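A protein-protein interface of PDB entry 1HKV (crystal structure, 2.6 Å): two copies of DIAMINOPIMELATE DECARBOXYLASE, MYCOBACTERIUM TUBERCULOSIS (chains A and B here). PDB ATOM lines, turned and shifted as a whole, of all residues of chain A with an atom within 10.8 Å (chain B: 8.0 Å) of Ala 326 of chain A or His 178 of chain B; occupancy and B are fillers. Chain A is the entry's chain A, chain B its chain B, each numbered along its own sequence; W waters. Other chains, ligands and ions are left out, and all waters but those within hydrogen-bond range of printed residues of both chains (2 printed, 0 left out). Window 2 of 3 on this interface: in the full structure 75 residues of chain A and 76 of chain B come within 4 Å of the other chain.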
ATOM      1  N   ASP A 321      -8.013  15.045  19.310  1.00  0.00           N
ATOM      2  CA  ASP A 321      -7.210  14.937  20.493  1.00  0.00           C
ATOM      3  C   ASP A 321      -7.145  13.513  20.855  1.00  0.00           C
ATOM      4  O   ASP A 321      -8.187  12.908  21.003  1.00  0.00           O
ATOM      5  CB  ASP A 321      -7.821  15.727  21.637  1.00  0.00           C
ATOM      6  CG  ASP A 321      -6.789  16.242  22.580  1.00  0.00           C
ATOM      7  OD1 ASP A 321      -6.950  16.004  23.829  1.00  0.00           O
ATOM      8  OD2 ASP A 321      -5.748  16.899  22.137  1.00  0.00           O
ATOM      9  N   VAL A 322      -5.928  12.933  20.915  1.00  0.00           N
ATOM     10  CA  VAL A 322      -5.784  11.505  21.218  1.00  0.00           C
ATOM     11  C   VAL A 322      -5.033  11.297  22.525  1.00  0.00           C
ATOM     12  O   VAL A 322      -3.978  11.800  22.704  1.00  0.00           O
ATOM     13  CB  VAL A 322      -5.115  10.692  20.020  1.00  0.00           C
ATOM     14  CG1 VAL A 322      -4.895   9.212  20.384  1.00  0.00           C
ATOM     15  CG2 VAL A 322      -5.945  10.758  18.818  1.00  0.00           C
ATOM     16  N   ASP A 323      -5.656  10.560  23.431  1.00  0.00           N
ATOM     17  CA  ASP A 323      -5.073  10.233  24.774  1.00  0.00           C
ATOM     18  C   ASP A 323      -4.060   9.142  24.637  1.00  0.00           C
ATOM     19  O   ASP A 323      -4.337   8.126  24.062  1.00  0.00           O
ATOM     20  CB  ASP A 323      -6.201   9.830  25.818  1.00  0.00           C
ATOM     21  CG  ASP A 323      -7.042   8.568  25.345  1.00  0.00           C
ATOM     22  OD1 ASP A 323      -7.029   7.497  26.079  1.00  0.00           O
ATOM     23  OD2 ASP A 323      -7.738   8.530  24.211  1.00  0.00           O
ATOM     24  N   VAL A 324      -2.862   9.410  25.139  1.00  0.00           N
ATOM     25  CA  VAL A 324      -1.703   8.550  24.998  1.00  0.00           C
ATOM     26  C   VAL A 324      -1.143   8.160  26.324  1.00  0.00           C
ATOM     27  O   VAL A 324      -0.188   7.467  26.380  1.00  0.00           O
ATOM     28  CB  VAL A 324      -0.505   9.266  24.243  1.00  0.00           C
ATOM     29  CG1 VAL A 324      -0.924   9.741  22.997  1.00  0.00           C
ATOM     30  CG2 VAL A 324       0.069  10.389  25.060  1.00  0.00           C
ATOM     31  N   SER A 325      -1.697   8.679  27.392  1.00  0.00           N
ATOM     32  CA  SER A 325      -1.412   8.173  28.746  1.00  0.00           C
ATOM     33  C   SER A 325      -2.504   8.596  29.641  1.00  0.00           C
ATOM     34  O   SER A 325      -3.514   9.021  29.193  1.00  0.00           O
ATOM     35  CB  SER A 325      -0.047   8.628  29.265  1.00  0.00           C
ATOM     36  OG  SER A 325      -0.082   9.904  29.811  1.00  0.00           O
ATOM     37  N   ALA A 326      -2.333   8.454  30.924  1.00  0.00           N
ATOM     38  CA  ALA A 326      -3.476   8.643  31.827  1.00  0.00           C
ATOM     39  C   ALA A 326      -3.702  10.093  31.993  1.00  0.00           C
ATOM     40  O   ALA A 326      -4.818  10.527  32.290  1.00  0.00           O
ATOM     41  CB  ALA A 326      -3.248   7.964  33.216  1.00  0.00           C
ATOM     42  N   THR A 327      -2.645  10.852  31.780  1.00  0.00           N
ATOM     43  CA  THR A 327      -2.700  12.317  31.900  1.00  0.00           C
ATOM     44  C   THR A 327      -2.514  13.055  30.521  1.00  0.00           C
ATOM     45  O   THR A 327      -3.235  14.000  30.227  1.00  0.00           O
ATOM     46  CB  THR A 327      -1.637  12.771  32.876  1.00  0.00           C
ATOM     47  OG1 THR A 327      -0.417  12.059  32.624  1.00  0.00           O
ATOM     48  CG2 THR A 327      -2.003  12.352  34.315  1.00  0.00           C
ATOM     49  N   ALA A 328      -1.606  12.546  29.676  1.00  0.00           N
ATOM     50  CA  ALA A 328      -1.190  13.224  28.443  1.00  0.00           C
ATOM     51  C   ALA A 328      -2.037  12.926  27.141  1.00  0.00           C
ATOM     52  O   ALA A 328      -2.742  11.888  26.998  1.00  0.00           O
ATOM     53  CB  ALA A 328       0.281  12.918  28.173  1.00  0.00           C
ATOM     54  N   HIS A 329      -1.933  13.864  26.220  1.00  0.00           N
ATOM     55  CA  HIS A 329      -2.604  13.789  24.943  1.00  0.00           C
ATOM     56  C   HIS A 329      -1.627  14.034  23.820  1.00  0.00           C
ATOM     57  O   HIS A 329      -0.475  14.439  24.054  1.00  0.00           O
ATOM     58  CB  HIS A 329      -3.709  14.809  24.895  1.00  0.00           C
ATOM     59  CG  HIS A 329      -4.748  14.602  25.951  1.00  0.00           C
ATOM     60  ND1 HIS A 329      -6.053  14.254  25.662  1.00  0.00           N
ATOM     61  CD2 HIS A 329      -4.665  14.646  27.301  1.00  0.00           C
ATOM     62  CE1 HIS A 329      -6.734  14.121  26.786  1.00  0.00           C
ATOM     63  NE2 HIS A 329      -5.912  14.345  27.795  1.00  0.00           N
ATOM     64  N   ARG A 330      -2.069  13.745  22.609  1.00  0.00           N
ATOM     65  CA  ARG A 330      -1.330  14.072  21.410  1.00  0.00           C
ATOM     66  C   ARG A 330      -2.309  14.594  20.386  1.00  0.00           C
ATOM     67  O   ARG A 330      -3.285  13.970  20.094  1.00  0.00           O
ATOM     68  CB  ARG A 330      -0.586  12.855  20.883  1.00  0.00           C
ATOM     69  CG  ARG A 330       0.320  13.127  19.665  1.00  0.00           C
ATOM     70  CD  ARG A 330       0.973  11.834  19.045  1.00  0.00           C
ATOM     71  NE  ARG A 330       1.289  10.891  20.095  1.00  0.00           N
ATOM     72  CZ  ARG A 330       2.284  11.042  20.941  1.00  0.00           C
ATOM     73  NH1 ARG A 330       3.086  12.070  20.870  1.00  0.00           N
ATOM     74  NH2 ARG A 330       2.459  10.167  21.856  1.00  0.00           N
ATOM     75  N   TYR A 332      -3.478  15.064  16.992  1.00  0.00           N
ATOM     76  CA  TYR A 332      -3.413  14.606  15.637  1.00  0.00           C
ATOM     77  C   TYR A 332      -4.077  15.594  14.669  1.00  0.00           C
ATOM     78  O   TYR A 332      -5.296  15.766  14.674  1.00  0.00           O
ATOM     79  CB  TYR A 332      -4.076  13.258  15.483  1.00  0.00           C
ATOM     80  CG  TYR A 332      -3.221  12.127  15.887  1.00  0.00           C
ATOM     81  CD1 TYR A 332      -3.003  11.845  17.226  1.00  0.00           C
ATOM     82  CD2 TYR A 332      -2.655  11.297  14.952  1.00  0.00           C
ATOM     83  CE1 TYR A 332      -2.256  10.786  17.602  1.00  0.00           C
ATOM     84  CE2 TYR A 332      -1.860  10.227  15.352  1.00  0.00           C
ATOM     85  CZ  TYR A 332      -1.671   9.990  16.670  1.00  0.00           C
ATOM     86  OH  TYR A 332      -0.934   8.948  17.082  1.00  0.00           O
ATOM     87  N   ARG A 369       0.958  15.387  16.143  1.00  0.00           N
ATOM     88  CA  ARG A 369       1.304  14.581  14.985  1.00  0.00           C
ATOM     89  C   ARG A 369       0.573  15.081  13.734  1.00  0.00           C
ATOM     90  O   ARG A 369      -0.637  15.060  13.694  1.00  0.00           O
ATOM     91  CB  ARG A 369       0.865  13.149  15.207  1.00  0.00           C
ATOM     92  CG  ARG A 369       2.018  12.190  15.576  1.00  0.00           C
ATOM     93  CD  ARG A 369       2.011  10.943  14.876  1.00  0.00           C
ATOM     94  NE  ARG A 369       2.132   9.783  15.747  1.00  0.00           N
ATOM     95  CZ  ARG A 369       3.007   9.584  16.757  1.00  0.00           C
ATOM     96  NH1 ARG A 369       3.889  10.468  17.134  1.00  0.00           N
ATOM     97  NH2 ARG A 369       2.950   8.440  17.414  1.00  0.00           N
ATOM     98  N   THR B 163     -11.510   2.618  18.610  1.00  0.00           N
ATOM     99  CA  THR B 163     -10.199   2.225  19.014  1.00  0.00           C
ATOM    100  C   THR B 163     -10.348   1.410  20.325  1.00  0.00           C
ATOM    101  O   THR B 163     -10.767   1.933  21.341  1.00  0.00           O
ATOM    102  CB  THR B 163      -9.450   3.483  19.192  1.00  0.00           C
ATOM    103  OG1 THR B 163      -8.700   3.697  18.037  1.00  0.00           O
ATOM    104  CG2 THR B 163      -8.457   3.452  20.246  1.00  0.00           C
ATOM    105  N   VAL B 164     -10.061   0.123  20.272  1.00  0.00           N
ATOM    106  CA  VAL B 164     -10.262  -0.728  21.427  1.00  0.00           C
ATOM    107  C   VAL B 164      -8.951  -1.142  22.066  1.00  0.00           C
ATOM    108  O   VAL B 164      -8.931  -1.968  22.891  1.00  0.00           O
ATOM    109  CB  VAL B 164     -11.102  -2.003  21.098  1.00  0.00           C
ATOM    110  CG1 VAL B 164     -12.472  -1.638  20.695  1.00  0.00           C
ATOM    111  CG2 VAL B 164     -10.479  -2.815  20.049  1.00  0.00           C
ATOM    112  N   GLY B 165      -7.858  -0.547  21.669  1.00  0.00           N
ATOM    113  CA  GLY B 165      -6.551  -0.877  22.267  1.00  0.00           C
ATOM    114  C   GLY B 165      -5.928  -2.260  21.934  1.00  0.00           C
ATOM    115  O   GLY B 165      -5.079  -2.794  22.696  1.00  0.00           O
ATOM    116  N   SER B 175      -1.907  -5.133  23.577  1.00  0.00           N
ATOM    117  CA  SER B 175      -3.017  -4.391  24.164  1.00  0.00           C
ATOM    118  C   SER B 175      -2.493  -3.091  24.835  1.00  0.00           C
ATOM    119  O   SER B 175      -1.376  -3.026  25.278  1.00  0.00           O
ATOM    120  CB  SER B 175      -3.696  -5.274  25.153  1.00  0.00           C
ATOM    121  OG  SER B 175      -4.725  -4.623  25.834  1.00  0.00           O
ATOM    122  N   THR B 176      -3.306  -2.044  24.834  1.00  0.00           N
ATOM    123  CA  THR B 176      -2.898  -0.734  25.386  1.00  0.00           C
ATOM    124  C   THR B 176      -4.007  -0.122  26.002  1.00  0.00           C
ATOM    125  O   THR B 176      -5.197  -0.277  25.582  1.00  0.00           O
ATOM    126  CB  THR B 176      -2.418   0.229  24.325  1.00  0.00           C
ATOM    127  OG1 THR B 176      -1.546  -0.440  23.484  1.00  0.00           O
ATOM    128  CG2 THR B 176      -1.536   1.344  24.928  1.00  0.00           C
ATOM    129  N   ALA B 177      -3.663   0.646  26.999  1.00  0.00           N
ATOM    130  CA  ALA B 177      -4.629   1.425  27.679  1.00  0.00           C
ATOM    131  C   ALA B 177      -5.041   2.589  26.736  1.00  0.00           C
ATOM    132  O   ALA B 177      -6.213   2.869  26.540  1.00  0.00           O
ATOM    133  CB  ALA B 177      -3.995   1.929  29.021  1.00  0.00           C
ATOM    134  N   HIS B 178      -4.058   3.209  26.121  1.00  0.00           N
ATOM    135  CA  HIS B 178      -4.308   4.360  25.273  1.00  0.00           C
ATOM    136  C   HIS B 178      -3.702   4.160  23.868  1.00  0.00           C
ATOM    137  O   HIS B 178      -2.525   4.343  23.666  1.00  0.00           O
ATOM    138  CB  HIS B 178      -3.755   5.625  25.967  1.00  0.00           C
ATOM    139  CG  HIS B 178      -4.205   5.772  27.404  1.00  0.00           C
ATOM    140  ND1 HIS B 178      -5.472   6.193  27.746  1.00  0.00           N
ATOM    141  CD2 HIS B 178      -3.571   5.503  28.576  1.00  0.00           C
ATOM    142  CE1 HIS B 178      -5.597   6.185  29.063  1.00  0.00           C
ATOM    143  NE2 HIS B 178      -4.454   5.780  29.591  1.00  0.00           N
ATOM    144  N   GLU B 179      -4.509   3.757  22.923  1.00  0.00           N
ATOM    145  CA  GLU B 179      -4.028   3.548  21.581  1.00  0.00           C
ATOM    146  C   GLU B 179      -3.665   4.891  20.960  1.00  0.00           C
ATOM    147  O   GLU B 179      -4.484   5.781  20.894  1.00  0.00           O
ATOM    148  CB  GLU B 179      -5.093   2.823  20.726  1.00  0.00           C
ATOM    149  CG  GLU B 179      -4.538   1.883  19.691  1.00  0.00           C
ATOM    150  CD  GLU B 179      -5.607   1.270  18.829  1.00  0.00           C
ATOM    151  OE1 GLU B 179      -6.463   0.527  19.355  1.00  0.00           O
ATOM    152  OE2 GLU B 179      -5.579   1.515  17.607  1.00  0.00           O
ATOM    153  N   ASP B 180      -2.440   5.000  20.497  1.00  0.00           N
ATOM    154  CA  ASP B 180      -1.872   6.225  20.027  1.00  0.00           C
ATOM    155  C   ASP B 180      -1.756   6.205  18.494  1.00  0.00           C
ATOM    156  O   ASP B 180      -0.756   6.004  17.974  1.00  0.00           O
ATOM    157  CB  ASP B 180      -0.509   6.353  20.661  1.00  0.00           C
ATOM    158  CG  ASP B 180       0.173   7.658  20.356  1.00  0.00           C
ATOM    159  OD1 ASP B 180       1.358   7.770  20.817  1.00  0.00           O
ATOM    160  OD2 ASP B 180      -0.363   8.615  19.664  1.00  0.00           O
ATOM    161  N   GLN B 181      -2.859   6.408  17.817  1.00  0.00           N
ATOM    162  CA  GLN B 181      -2.900   6.463  16.349  1.00  0.00           C
ATOM    163  C   GLN B 181      -4.057   7.372  15.936  1.00  0.00           C
ATOM    164  O   GLN B 181      -4.883   7.781  16.770  1.00  0.00           O
ATOM    165  CB  GLN B 181      -3.124   5.070  15.785  1.00  0.00           C
ATOM    166  CG  GLN B 181      -4.531   4.523  16.049  1.00  0.00           C
ATOM    167  CD  GLN B 181      -5.071   3.768  14.894  1.00  0.00           C
ATOM    168  OE1 GLN B 181      -4.938   4.199  13.756  1.00  0.00           O
ATOM    169  NE2 GLN B 181      -5.705   2.641  15.163  1.00  0.00           N
ATOM    170  N   SER B 186     -11.625   6.399  20.829  1.00  0.00           N
ATOM    171  CA  SER B 186     -11.313   5.481  21.890  1.00  0.00           C
ATOM    172  C   SER B 186     -12.562   5.088  22.678  1.00  0.00           C
ATOM    173  O   SER B 186     -13.307   5.920  23.078  1.00  0.00           O
ATOM    174  CB  SER B 186     -10.291   6.093  22.838  1.00  0.00           C
ATOM    175  OG  SER B 186     -10.219   5.301  24.029  1.00  0.00           O
ATOM    176  N   ALA B 188     -12.277   3.249  25.697  1.00  0.00           N
ATOM    177  CA  ALA B 188     -11.890   3.413  27.077  1.00  0.00           C
ATOM    178  C   ALA B 188     -11.969   4.832  27.568  1.00  0.00           C
ATOM    179  O   ALA B 188     -12.045   5.024  28.709  1.00  0.00           O
ATOM    180  CB  ALA B 188     -10.511   2.914  27.291  1.00  0.00           C
ATOM    181  N   SER B 189     -11.879   5.811  26.697  1.00  0.00           N
ATOM    182  CA  SER B 189     -11.738   7.198  27.121  1.00  0.00           C
ATOM    183  C   SER B 189     -13.117   7.807  27.197  1.00  0.00           C
ATOM    184  O   SER B 189     -13.273   8.874  27.704  1.00  0.00           O
ATOM    185  CB  SER B 189     -10.869   8.015  26.121  1.00  0.00           C
ATOM    186  OG  SER B 189     -11.524   8.202  24.838  1.00  0.00           O
ATOM    187  N   ARG B 230     -14.111  -6.082  23.567  1.00  0.00           N
ATOM    188  CA  ARG B 230     -14.114  -4.696  23.918  1.00  0.00           C
ATOM    189  C   ARG B 230     -15.167  -3.979  23.096  1.00  0.00           C
ATOM    190  O   ARG B 230     -15.879  -3.119  23.617  1.00  0.00           O
ATOM    191  CB  ARG B 230     -12.758  -4.097  23.677  1.00  0.00           C
ATOM    192  CG  ARG B 230     -11.892  -4.004  24.875  1.00  0.00           C
ATOM    193  CD  ARG B 230     -10.741  -4.980  24.874  1.00  0.00           C
ATOM    194  NE  ARG B 230      -9.441  -4.349  24.608  1.00  0.00           N
ATOM    195  CZ  ARG B 230      -8.351  -4.473  25.368  1.00  0.00           C
ATOM    196  NH1 ARG B 230      -8.341  -5.196  26.467  1.00  0.00           N
ATOM    197  NH2 ARG B 230      -7.252  -3.892  25.001  1.00  0.00           N
HETATM  198  O   HOH W   1      -6.361   6.423  22.807  1.00  0.00           O
HETATM  199  O   HOH W   2       4.481   7.472  19.972  1.00  0.00           O
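Water W1 bridges the backbone carbonyl oxygen (O) of Glu 179 of chain B and the side-chain carboxylate (OD2) of Asp 323 of chain A.
Water W2 lies within hydrogen-bond range of NH2 of Arg 369 of chain A and OD1 of Asp 180 of chain B.
Among the printed residues, pairs that only touch across the chains: Val 322 of chain A with Glu 179 of chain B, Val 324 of chain A with Asp 180 of chain B, Val 324 of chain A with His 178 of chain B, Ala 326 of chain A with His 178 of chain B, Asp 323 of chain A with Ser 189 of chain B, Val 322 of chain A with Gln 181 of chain B, Asp 323 of chain A with Ser 186 of chain B and Asp 323 of chain A with Glu 179 of chain B.
Of the 12 printed residues of chain A, 8 touch a printed residue of chain B.
Among the printed residues, 14 pairs touch across the chains.
The side-chain carboxylate (OD1) of Asp 323 of chain A sits at hydrogen-bond distance from a ring nitrogen (ND1) of His 178 of chain B, 2.6 Å away.
A ring nitrogen (NE2) of His 178 of chain B lies within hydrogen-bond range of the backbone carbonyl oxygen of Ser 325 of chain A (3.4 Å).
The guanidinium group (NH2) of Arg 330 of chain A lies within salt-bridge range of the side-chain carboxylate (OD1) of Asp 180 of chain B (2.8 Å).
OH of Tyr 332 of chain A is in hydrogen-bond range of OD2 of Asp 180 of chain B, at 2.7 Å.
The side-chain hydroxyl of Tyr 332 of chain A sits close to the backbone NH of Gln 181 of chain B.
NH2 of Arg 369 of chain A is in salt-bridge range of OD1 of Asp 180 of chain B (3.8 Å).
Ala 326 of chain A touches just one residue of chain B: His 178.
His 178 of chain B touches just these residues of chain A: Asp 323 (2.6 Å), Val 324 (3.7 Å), Ser 325 (3.4 Å) and Ala 326 (3.7 Å).
No residue of chain A comes within 4 Å of Thr 176 of chain B.
Of the printed residues of chain B, Arg 330 of chain A touches Asp 180 (2.8 Å).
Printed residues of chain B within 4 Å of Val 324 of chain A: His 178 (3.7 Å) and Asp 180 (3.5 Å).
Of the printed residues of chain A, Ser 189 of chain B touches Asp 323.
Of the printed residues of chain B, Asp 323 of chain A touches His 178, Glu 179, Ser 186 and Ser 189.
Ala 328 of chain A touches none of the printed residues of chain B.
The nearest residue of chain B that does not touch Ala 326 of chain A is Ala 177 of chain B (7.0 Å).
No position is printed for both chains.
The backbone NH (N) of Arg 330 of chain A is in hydrogen-bond range of the backbone carbonyl oxygen (O) of Val 322 of chain A, at 2.7 Å.
The side-chain hydroxyl (OG) of Ser 325 of chain A lies close to the backbone NH (N) of Thr 327 of chain A (3.4 Å).
OG of Ser 325 of chain A sits at hydrogen-bond distance from N of Ala 328 of chain A (3.1 Å).
NE of Arg 369 of chain A is in hydrogen-bond range of OH of Tyr 332 of chain A, at 3.4 Å.
The side-chain hydroxyl of Ser 186 of chain B is in hydrogen-bond range of the backbone NH of Ala 188 of chain B (3.4 Å).
The side-chain hydroxyl (OG) of Ser 186 of chain B lies within hydrogen-bond range of the backbone NH (N) of Ser 189 of chain B (3.2 Å).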
